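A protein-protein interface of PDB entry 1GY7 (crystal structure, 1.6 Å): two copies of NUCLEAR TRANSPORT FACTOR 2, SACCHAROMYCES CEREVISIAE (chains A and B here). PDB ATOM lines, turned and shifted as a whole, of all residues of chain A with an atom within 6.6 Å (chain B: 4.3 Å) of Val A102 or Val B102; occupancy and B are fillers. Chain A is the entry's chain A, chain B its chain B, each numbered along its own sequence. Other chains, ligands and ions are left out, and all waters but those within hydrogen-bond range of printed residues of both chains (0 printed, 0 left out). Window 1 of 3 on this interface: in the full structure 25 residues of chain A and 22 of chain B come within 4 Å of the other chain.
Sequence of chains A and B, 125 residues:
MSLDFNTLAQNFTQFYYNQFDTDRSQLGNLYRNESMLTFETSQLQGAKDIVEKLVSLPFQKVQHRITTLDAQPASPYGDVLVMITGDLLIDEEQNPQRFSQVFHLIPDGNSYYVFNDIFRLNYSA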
ATOM      1  N   TYR A  17       1.396 -27.206  14.979  1.00  0.00           N
ATOM      2  CA  TYR A  17       1.180 -25.766  14.993  1.00  0.00           C
ATOM      3  C   TYR A  17       0.241 -25.317  16.103  1.00  0.00           C
ATOM      4  O   TYR A  17       0.422 -24.240  16.669  1.00  0.00           O
ATOM      5  CB  TYR A  17       0.679 -25.284  13.628  1.00  0.00           C
ATOM      6  CG  TYR A  17       1.738 -25.375  12.544  1.00  0.00           C
ATOM      7  CD1 TYR A  17       3.034 -24.911  12.770  1.00  0.00           C
ATOM      8  CD2 TYR A  17       1.439 -25.905  11.293  1.00  0.00           C
ATOM      9  CE1 TYR A  17       4.007 -24.970  11.771  1.00  0.00           C
ATOM     10  CE2 TYR A  17       2.401 -25.963  10.288  1.00  0.00           C
ATOM     11  CZ  TYR A  17       3.681 -25.495  10.533  1.00  0.00           C
ATOM     12  OH  TYR A  17       4.615 -25.537   9.519  1.00  0.00           O
ATOM     13  N   GLN A  72       4.695 -36.450   1.028  1.00  0.00           N
ATOM     14  CA  GLN A  72       5.094 -37.598   0.219  1.00  0.00           C
ATOM     15  C   GLN A  72       5.816 -38.579   1.123  1.00  0.00           C
ATOM     16  O   GLN A  72       6.408 -38.190   2.131  1.00  0.00           O
ATOM     17  CB  GLN A  72       6.090 -37.212  -0.884  1.00  0.00           C
ATOM     18  CG  GLN A  72       5.606 -36.237  -1.936  1.00  0.00           C
ATOM     19  CD  GLN A  72       6.678 -35.954  -2.981  1.00  0.00           C
ATOM     20  OE1 GLN A  72       7.855 -36.289  -2.791  1.00  0.00           O
ATOM     21  NE2 GLN A  72       6.279 -35.326  -4.085  1.00  0.00           N
ATOM     22  N   LEU A  81       7.646 -36.885   4.339  1.00  0.00           N
ATOM     23  CA  LEU A  81       8.202 -35.562   4.103  1.00  0.00           C
ATOM     24  C   LEU A  81       6.996 -34.640   3.933  1.00  0.00           C
ATOM     25  O   LEU A  81       6.072 -34.954   3.184  1.00  0.00           O
ATOM     26  CB  LEU A  81       9.052 -35.569   2.830  1.00  0.00           C
ATOM     27  CG  LEU A  81       9.873 -34.314   2.538  1.00  0.00           C
ATOM     28  CD1 LEU A  81      10.818 -34.052   3.700  1.00  0.00           C
ATOM     29  CD2 LEU A  81      10.653 -34.499   1.240  1.00  0.00           C
ATOM     30  N   VAL A  82       6.995 -33.516   4.640  1.00  0.00           N
ATOM     31  CA  VAL A  82       5.887 -32.567   4.543  1.00  0.00           C
ATOM     32  C   VAL A  82       6.413 -31.162   4.305  1.00  0.00           C
ATOM     33  O   VAL A  82       7.310 -30.709   5.017  1.00  0.00           O
ATOM     34  CB  VAL A  82       5.054 -32.529   5.845  1.00  0.00           C
ATOM     35  CG1 VAL A  82       3.854 -31.604   5.665  1.00  0.00           C
ATOM     36  CG2 VAL A  82       4.618 -33.930   6.233  1.00  0.00           C
ATOM     37  N   MET A  83       5.878 -30.476   3.298  1.00  0.00           N
ATOM     38  CA  MET A  83       6.290 -29.101   3.045  1.00  0.00           C
ATOM     39  C   MET A  83       5.089 -28.213   3.299  1.00  0.00           C
ATOM     40  O   MET A  83       3.983 -28.502   2.847  1.00  0.00           O
ATOM     41  CB  MET A  83       6.781 -28.887   1.609  1.00  0.00           C
ATOM     42  CG  MET A  83       7.280 -27.463   1.383  1.00  0.00           C
ATOM     43  SD  MET A  83       8.006 -27.124  -0.247  1.00  0.00           S
ATOM     44  CE  MET A  83       6.546 -26.630  -1.172  1.00  0.00           C
ATOM     45  N   ILE A  84       5.320 -27.126   4.019  1.00  0.00           N
ATOM     46  CA  ILE A  84       4.258 -26.192   4.363  1.00  0.00           C
ATOM     47  C   ILE A  84       4.648 -24.761   4.009  1.00  0.00           C
ATOM     48  O   ILE A  84       5.814 -24.383   4.099  1.00  0.00           O
ATOM     49  CB  ILE A  84       3.983 -26.211   5.897  1.00  0.00           C
ATOM     50  CG1 ILE A  84       3.666 -27.631   6.366  1.00  0.00           C
ATOM     51  CG2 ILE A  84       2.859 -25.248   6.254  1.00  0.00           C
ATOM     52  CD1 ILE A  84       4.863 -28.363   6.948  1.00  0.00           C
ATOM     53  N   SER A 100       7.976 -20.714   5.097  1.00  0.00           N
ATOM     54  CA  SER A 100       8.057 -21.987   4.390  1.00  0.00           C
ATOM     55  C   SER A 100       8.700 -22.922   5.403  1.00  0.00           C
ATOM     56  O   SER A 100       9.624 -22.530   6.117  1.00  0.00           O
ATOM     57  CB  SER A 100       8.934 -21.878   3.138  1.00  0.00           C
ATOM     58  OG  SER A 100       8.306 -21.084   2.138  1.00  0.00           O
ATOM     59  N   GLN A 101       8.207 -24.148   5.486  1.00  0.00           N
ATOM     60  CA  GLN A 101       8.754 -25.091   6.450  1.00  0.00           C
ATOM     61  C   GLN A 101       8.675 -26.508   5.920  1.00  0.00           C
ATOM     62  O   GLN A 101       7.749 -26.856   5.191  1.00  0.00           O
ATOM     63  CB  GLN A 101       7.973 -24.987   7.768  1.00  0.00           C
ATOM     64  CG  GLN A 101       8.508 -25.871   8.892  1.00  0.00           C
ATOM     65  CD  GLN A 101       8.155 -25.344  10.277  1.00  0.00           C
ATOM     66  OE1 GLN A 101       8.879 -25.583  11.245  1.00  0.00           O
ATOM     67  NE2 GLN A 101       7.042 -24.634  10.377  1.00  0.00           N
ATOM     68  N   VAL A 102       9.669 -27.316   6.256  1.00  0.00           N
ATOM     69  CA  VAL A 102       9.654 -28.706   5.848  1.00  0.00           C
ATOM     70  C   VAL A 102       9.943 -29.574   7.069  1.00  0.00           C
ATOM     71  O   VAL A 102      10.788 -29.234   7.900  1.00  0.00           O
ATOM     72  CB  VAL A 102      10.687 -29.004   4.733  1.00  0.00           C
ATOM     73  CG1 VAL A 102      12.081 -28.633   5.187  1.00  0.00           C
ATOM     74  CG2 VAL A 102      10.618 -30.490   4.356  1.00  0.00           C
ATOM     75  N   PHE A 103       9.193 -30.666   7.189  1.00  0.00           N
ATOM     76  CA  PHE A 103       9.352 -31.627   8.279  1.00  0.00           C
ATOM     77  C   PHE A 103       9.615 -33.007   7.697  1.00  0.00           C
ATOM     78  O   PHE A 103       9.013 -33.386   6.691  1.00  0.00           O
ATOM     79  CB  PHE A 103       8.067 -31.780   9.112  1.00  0.00           C
ATOM     80  CG  PHE A 103       7.684 -30.572   9.913  1.00  0.00           C
ATOM     81  CD1 PHE A 103       6.451 -29.967   9.714  1.00  0.00           C
ATOM     82  CD2 PHE A 103       8.519 -30.078  10.905  1.00  0.00           C
ATOM     83  CE1 PHE A 103       6.050 -28.887  10.490  1.00  0.00           C
ATOM     84  CE2 PHE A 103       8.128 -28.998  11.690  1.00  0.00           C
ATOM     85  CZ  PHE A 103       6.890 -28.399  11.482  1.00  0.00           C
ATOM     86  N   HIS A 104      10.524 -33.749   8.319  1.00  0.00           N
ATOM     87  CA  HIS A 104      10.781 -35.129   7.924  1.00  0.00           C
ATOM     88  C   HIS A 104      10.292 -35.841   9.186  1.00  0.00           C
ATOM     89  O   HIS A 104      10.898 -35.724  10.251  1.00  0.00           O
ATOM     90  CB  HIS A 104      12.274 -35.369   7.683  1.00  0.00           C
ATOM     91  CG  HIS A 104      12.625 -36.779   7.307  1.00  0.00           C
ATOM     92  ND1 HIS A 104      11.674 -37.743   7.044  1.00  0.00           N
ATOM     93  CD2 HIS A 104      13.824 -37.378   7.148  1.00  0.00           C
ATOM     94  CE1 HIS A 104      12.283 -38.883   6.740  1.00  0.00           C
ATOM     95  NE2 HIS A 104      13.584 -38.687   6.796  1.00  0.00           N
ATOM     96  N   VAL A 114       9.606 -35.442  14.936  1.00  0.00           N
ATOM     97  CA  VAL A 114      10.279 -34.660  13.904  1.00  0.00           C
ATOM     98  C   VAL A 114      11.787 -34.900  13.879  1.00  0.00           C
ATOM     99  O   VAL A 114      12.476 -34.634  14.864  1.00  0.00           O
ATOM    100  CB  VAL A 114      10.015 -33.152  14.124  1.00  0.00           C
ATOM    101  CG1 VAL A 114      10.719 -32.329  13.052  1.00  0.00           C
ATOM    102  CG2 VAL A 114       8.511 -32.883  14.111  1.00  0.00           C
ATOM    103  N   ASN A 116      13.784 -33.917  10.901  1.00  0.00           N
ATOM    104  CA  ASN A 116      14.283 -32.704  10.246  1.00  0.00           C
ATOM    105  C   ASN A 116      13.207 -31.635  10.337  1.00  0.00           C
ATOM    106  O   ASN A 116      12.034 -31.908  10.088  1.00  0.00           O
ATOM    107  CB  ASN A 116      14.557 -32.903   8.751  1.00  0.00           C
ATOM    108  CG  ASN A 116      15.665 -33.882   8.475  1.00  0.00           C
ATOM    109  OD1 ASN A 116      16.838 -33.632   8.771  1.00  0.00           O
ATOM    110  ND2 ASN A 116      15.306 -35.002   7.884  1.00  0.00           N
ATOM    111  N   ASP A 117      13.622 -30.423  10.678  1.00  0.00           N
ATOM    112  CA  ASP A 117      12.728 -29.279  10.761  1.00  0.00           C
ATOM    113  C   ASP A 117      13.528 -28.120  10.177  1.00  0.00           C
ATOM    114  O   ASP A 117      14.540 -27.712  10.752  1.00  0.00           O
ATOM    115  CB  ASP A 117      12.363 -28.978  12.218  1.00  0.00           C
ATOM    116  CG  ASP A 117      11.446 -27.774  12.358  1.00  0.00           C
ATOM    117  OD1 ASP A 117      11.231 -27.065  11.352  1.00  0.00           O
ATOM    118  OD2 ASP A 117      10.944 -27.529  13.480  1.00  0.00           O
ATOM    119  N   ILE A 118      13.113 -27.635   9.008  1.00  0.00           N
ATOM    120  CA  ILE A 118      13.780 -26.503   8.370  1.00  0.00           C
ATOM    121  C   ILE A 118      12.728 -25.412   8.229  1.00  0.00           C
ATOM    122  O   ILE A 118      11.674 -25.635   7.635  1.00  0.00           O
ATOM    123  CB  ILE A 118      14.332 -26.869   6.982  1.00  0.00           C
ATOM    124  CG1 ILE A 118      15.326 -28.030   7.118  1.00  0.00           C
ATOM    125  CG2 ILE A 118      15.023 -25.646   6.362  1.00  0.00           C
ATOM    126  CD1 ILE A 118      15.813 -28.608   5.794  1.00  0.00           C
ATOM    127  N   PHE A 119      13.023 -24.239   8.777  1.00  0.00           N
ATOM    128  CA  PHE A 119      12.078 -23.127   8.762  1.00  0.00           C
ATOM    129  C   PHE A 119      12.672 -21.823   8.238  1.00  0.00           C
ATOM    130  O   PHE A 119      13.778 -21.425   8.612  1.00  0.00           O
ATOM    131  CB  PHE A 119      11.549 -22.916  10.182  1.00  0.00           C
ATOM    132  CG  PHE A 119      10.647 -21.721  10.333  1.00  0.00           C
ATOM    133  CD1 PHE A 119       9.281 -21.827  10.102  1.00  0.00           C
ATOM    134  CD2 PHE A 119      11.169 -20.488  10.719  1.00  0.00           C
ATOM    135  CE1 PHE A 119       8.438 -20.717  10.255  1.00  0.00           C
ATOM    136  CE2 PHE A 119      10.339 -19.376  10.874  1.00  0.00           C
ATOM    137  CZ  PHE A 119       8.973 -19.489  10.642  1.00  0.00           C
ATOM    138  N   LEU B  81      18.317 -33.493   2.725  1.00  0.00           N
ATOM    139  CA  LEU B  81      17.040 -32.811   2.591  1.00  0.00           C
ATOM    140  C   LEU B  81      17.379 -31.343   2.369  1.00  0.00           C
ATOM    141  O   LEU B  81      18.178 -30.768   3.111  1.00  0.00           O
ATOM    142  CB  LEU B  81      16.228 -32.953   3.871  1.00  0.00           C
ATOM    143  CG  LEU B  81      14.855 -32.290   3.837  1.00  0.00           C
ATOM    144  CD1 LEU B  81      13.959 -33.065   2.882  1.00  0.00           C
ATOM    145  CD2 LEU B  81      14.263 -32.272   5.240  1.00  0.00           C
ATOM    146  N   VAL B  82      16.792 -30.738   1.345  1.00  0.00           N
ATOM    147  CA  VAL B  82      17.066 -29.333   1.081  1.00  0.00           C
ATOM    148  C   VAL B  82      15.798 -28.574   0.752  1.00  0.00           C
ATOM    149  O   VAL B  82      14.957 -29.046  -0.019  1.00  0.00           O
ATOM    150  CB  VAL B  82      18.075 -29.165  -0.081  1.00  0.00           C
ATOM    151  CG1 VAL B  82      17.544 -29.836  -1.338  1.00  0.00           C
ATOM    152  CG2 VAL B  82      18.348 -27.682  -0.328  1.00  0.00           C
ATOM    153  N   MET B  83      15.653 -27.404   1.362  1.00  0.00           N
ATOM    154  CA  MET B  83      14.497 -26.560   1.100  1.00  0.00           C
ATOM    155  C   MET B  83      15.020 -25.286   0.452  1.00  0.00           C
ATOM    156  O   MET B  83      15.981 -24.683   0.932  1.00  0.00           O
ATOM    157  CB  MET B  83      13.746 -26.226   2.389  1.00  0.00           C
ATOM    158  CG  MET B  83      12.500 -25.392   2.128  1.00  0.00           C
ATOM    159  SD  MET B  83      11.570 -25.004   3.614  1.00  0.00           S
ATOM    160  CE  MET B  83      12.506 -23.619   4.247  1.00  0.00           C
ATOM    161  N   GLN B 101      10.562 -24.919  -2.793  1.00  0.00           N
ATOM    162  CA  GLN B 101      10.766 -26.286  -3.254  1.00  0.00           C
ATOM    163  C   GLN B 101      11.570 -27.105  -2.259  1.00  0.00           C
ATOM    164  O   GLN B 101      12.442 -26.584  -1.562  1.00  0.00           O
ATOM    165  CB  GLN B 101      11.491 -26.281  -4.610  1.00  0.00           C
ATOM    166  CG  GLN B 101      11.659 -27.660  -5.243  1.00  0.00           C
ATOM    167  CD  GLN B 101      11.926 -27.595  -6.744  1.00  0.00           C
ATOM    168  OE1 GLN B 101      11.622 -28.535  -7.485  1.00  0.00           O
ATOM    169  NE2 GLN B 101      12.499 -26.490  -7.196  1.00  0.00           N
ATOM    170  N   VAL B 102      11.252 -28.391  -2.174  1.00  0.00           N
ATOM    171  CA  VAL B 102      11.992 -29.288  -1.300  1.00  0.00           C
ATOM    172  C   VAL B 102      12.450 -30.495  -2.106  1.00  0.00           C
ATOM    173  O   VAL B 102      11.690 -31.041  -2.908  1.00  0.00           O
ATOM    174  CB  VAL B 102      11.133 -29.787  -0.110  1.00  0.00           C
ATOM    175  CG1 VAL B 102      11.778 -31.019   0.522  1.00  0.00           C
ATOM    176  CG2 VAL B 102      11.000 -28.692   0.926  1.00  0.00           C
ATOM    177  N   PHE B 103      13.705 -30.886  -1.906  1.00  0.00           N
ATOM    178  CA  PHE B 103      14.267 -32.062  -2.562  1.00  0.00           C
ATOM    179  C   PHE B 103      14.794 -32.999  -1.487  1.00  0.00           C
ATOM    180  O   PHE B 103      15.352 -32.546  -0.486  1.00  0.00           O
ATOM    181  CB  PHE B 103      15.484 -31.729  -3.430  1.00  0.00           C
ATOM    182  CG  PHE B 103      15.189 -30.914  -4.651  1.00  0.00           C
ATOM    183  CD1 PHE B 103      15.793 -29.671  -4.820  1.00  0.00           C
ATOM    184  CD2 PHE B 103      14.391 -31.416  -5.670  1.00  0.00           C
ATOM    185  CE1 PHE B 103      15.610 -28.942  -5.992  1.00  0.00           C
ATOM    186  CE2 PHE B 103      14.205 -30.690  -6.848  1.00  0.00           C
ATOM    187  CZ  PHE B 103      14.818 -29.454  -7.005  1.00  0.00           C
ATOM    188  N   ASN B 116      12.367 -37.283  -3.713  1.00  0.00           N
ATOM    189  CA  ASN B 116      11.185 -36.477  -3.417  1.00  0.00           C
ATOM    190  C   ASN B 116      11.417 -35.077  -3.957  1.00  0.00           C
ATOM    191  O   ASN B 116      12.484 -34.494  -3.762  1.00  0.00           O
ATOM    192  CB  ASN B 116      10.942 -36.343  -1.913  1.00  0.00           C
ATOM    193  CG  ASN B 116      10.569 -37.644  -1.267  1.00  0.00           C
ATOM    194  OD1 ASN B 116       9.485 -38.190  -1.503  1.00  0.00           O
ATOM    195  ND2 ASN B 116      11.463 -38.155  -0.435  1.00  0.00           N
ATOM    196  N   ASP B 117      10.406 -34.547  -4.628  1.00  0.00           N
ATOM    197  CA  ASP B 117      10.454 -33.208  -5.187  1.00  0.00           C
ATOM    198  C   ASP B 117       9.075 -32.611  -4.926  1.00  0.00           C
ATOM    199  O   ASP B 117       8.075 -33.119  -5.427  1.00  0.00           O
ATOM    200  CB  ASP B 117      10.719 -33.279  -6.696  1.00  0.00           C
ATOM    201  CG  ASP B 117      10.825 -31.907  -7.348  1.00  0.00           C
ATOM    202  OD1 ASP B 117      10.404 -30.903  -6.732  1.00  0.00           O
ATOM    203  OD2 ASP B 117      11.324 -31.840  -8.496  1.00  0.00           O
ATOM    204  N   ILE B 118       9.020 -31.556  -4.121  1.00  0.00           N
ATOM    205  CA  ILE B 118       7.752 -30.887  -3.828  1.00  0.00           C
ATOM    206  C   ILE B 118       7.921 -29.431  -4.236  1.00  0.00           C
ATOM    207  O   ILE B 118       8.842 -28.754  -3.780  1.00  0.00           O
ATOM    208  CB  ILE B 118       7.404 -30.966  -2.342  1.00  0.00           C
ATOM    209  CG1 ILE B 118       7.274 -32.433  -1.923  1.00  0.00           C
ATOM    210  CG2 ILE B 118       6.096 -30.209  -2.077  1.00  0.00           C
ATOM    211  CD1 ILE B 118       6.981 -32.615  -0.437  1.00  0.00           C
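The side-chain carboxylate (OD1) of Asp A117 lies close to the side-chain amide oxygen (OE1) of Gln A101. The backbone carbonyl oxygen (O) of Gln A101 lies within hydrogen-bond range of the backbone NH (N) of Ile A84, at 2.7 Å. O of Ile A118 sits at hydrogen-bond distance from N of Val A102, at 3.0 Å. N of Val B102 lies within hydrogen-bond range of O of Ile B118. The backbone carbonyl oxygen of Asn A116 is in hydrogen-bond range of the backbone NH of His A104. The side-chain hydroxyl (OH) of Tyr A17 lies within hydrogen-bond range of the side-chain amide nitrogen (NE2) of Gln A101 (2.7 Å).
Ile B118 touches Gln A72 (CG1 to CD, 3.7 Å). Leu B81 touches Leu A81 (CD1 to CD1, 3.4 Å). Leu A81 touches Val B102. Met A83 touches Ile B118 (CE to CG2, 3.7 Å). Met B83 touches Ser A100 (CE to O, 3.6 Å). N of Gln A101 touches SD of Met B83, 3.9 Å away. Met B83 touches Val A102 (SD to CG1, 3.99 Å). CG2 of Val B102 touches CB of Val A102, 3.8 Å away. CB of Asn A116 touches CD2 of Leu B81, 3.6 Å away. Ile A118 touches Met B83 (CG2 to CE, 3.9 Å).
Of the 16 printed residues of chain A, 8 touch a printed residue of chain B. Printed residues of chain A that touch a printed residue of chain B: Gln A72, Leu A81, Met A83, Ser A100, Gln A101, Val A102, Asn A116 and Ile A118. Hydrophobic or aromatic side chains of chain A that line the printed part of chain B: Leu A81, Met A83, Val A102 and Ile A118. Among the printed residues, no Asp or Glu carboxylate lies within 4 Å of a Lys or Arg side-chain nitrogen of the other chain.
Of the printed residues of chain B, Val A102 touches Met B83 (3.99 Å) and Val B102 (3.8 Å). Of chain A, only Leu A81 (3.7 Å), Met A83 (3.6 Å) and Val A102 (3.8 Å) come within 4 Å of Val B102. Of the printed residues of chain B, Ile A118 touches Met B83. Printed residues of chain A within 4 Å of Asn B116: Gln A72 and Leu A81. Printed residues of chain B within 4 Å of Ser A100: Met B83. Val B82 touches none of the printed residues of chain A. Phe B103 touches none of the printed residues of chain A. The nearest residue of chain A that does not touch Val B102 is Gln A101 (5.7 Å).
NE2 of Gln A72 is in hydrogen-bond range of O of Asp B117 (3.1 Å). OE1 of Gln A72 lies close to OD1 of Asn B116, 2.8 Å away.
Leu A81 touches its own counterpart, Leu B81. Leu A81 touches Asn B116, and with the chains exchanged Asn A116 touches Leu B81. Met A83 touches Ile B118, and with the chains exchanged Ile A118 touches Met B83. Gln A101 touches Met B83, but with the chains exchanged Met A83 does not touch Gln B101 (4.1 Å). Positions printed for both chains: 81, 82, 83, 101, 102, 103, 116, 117 and 118.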
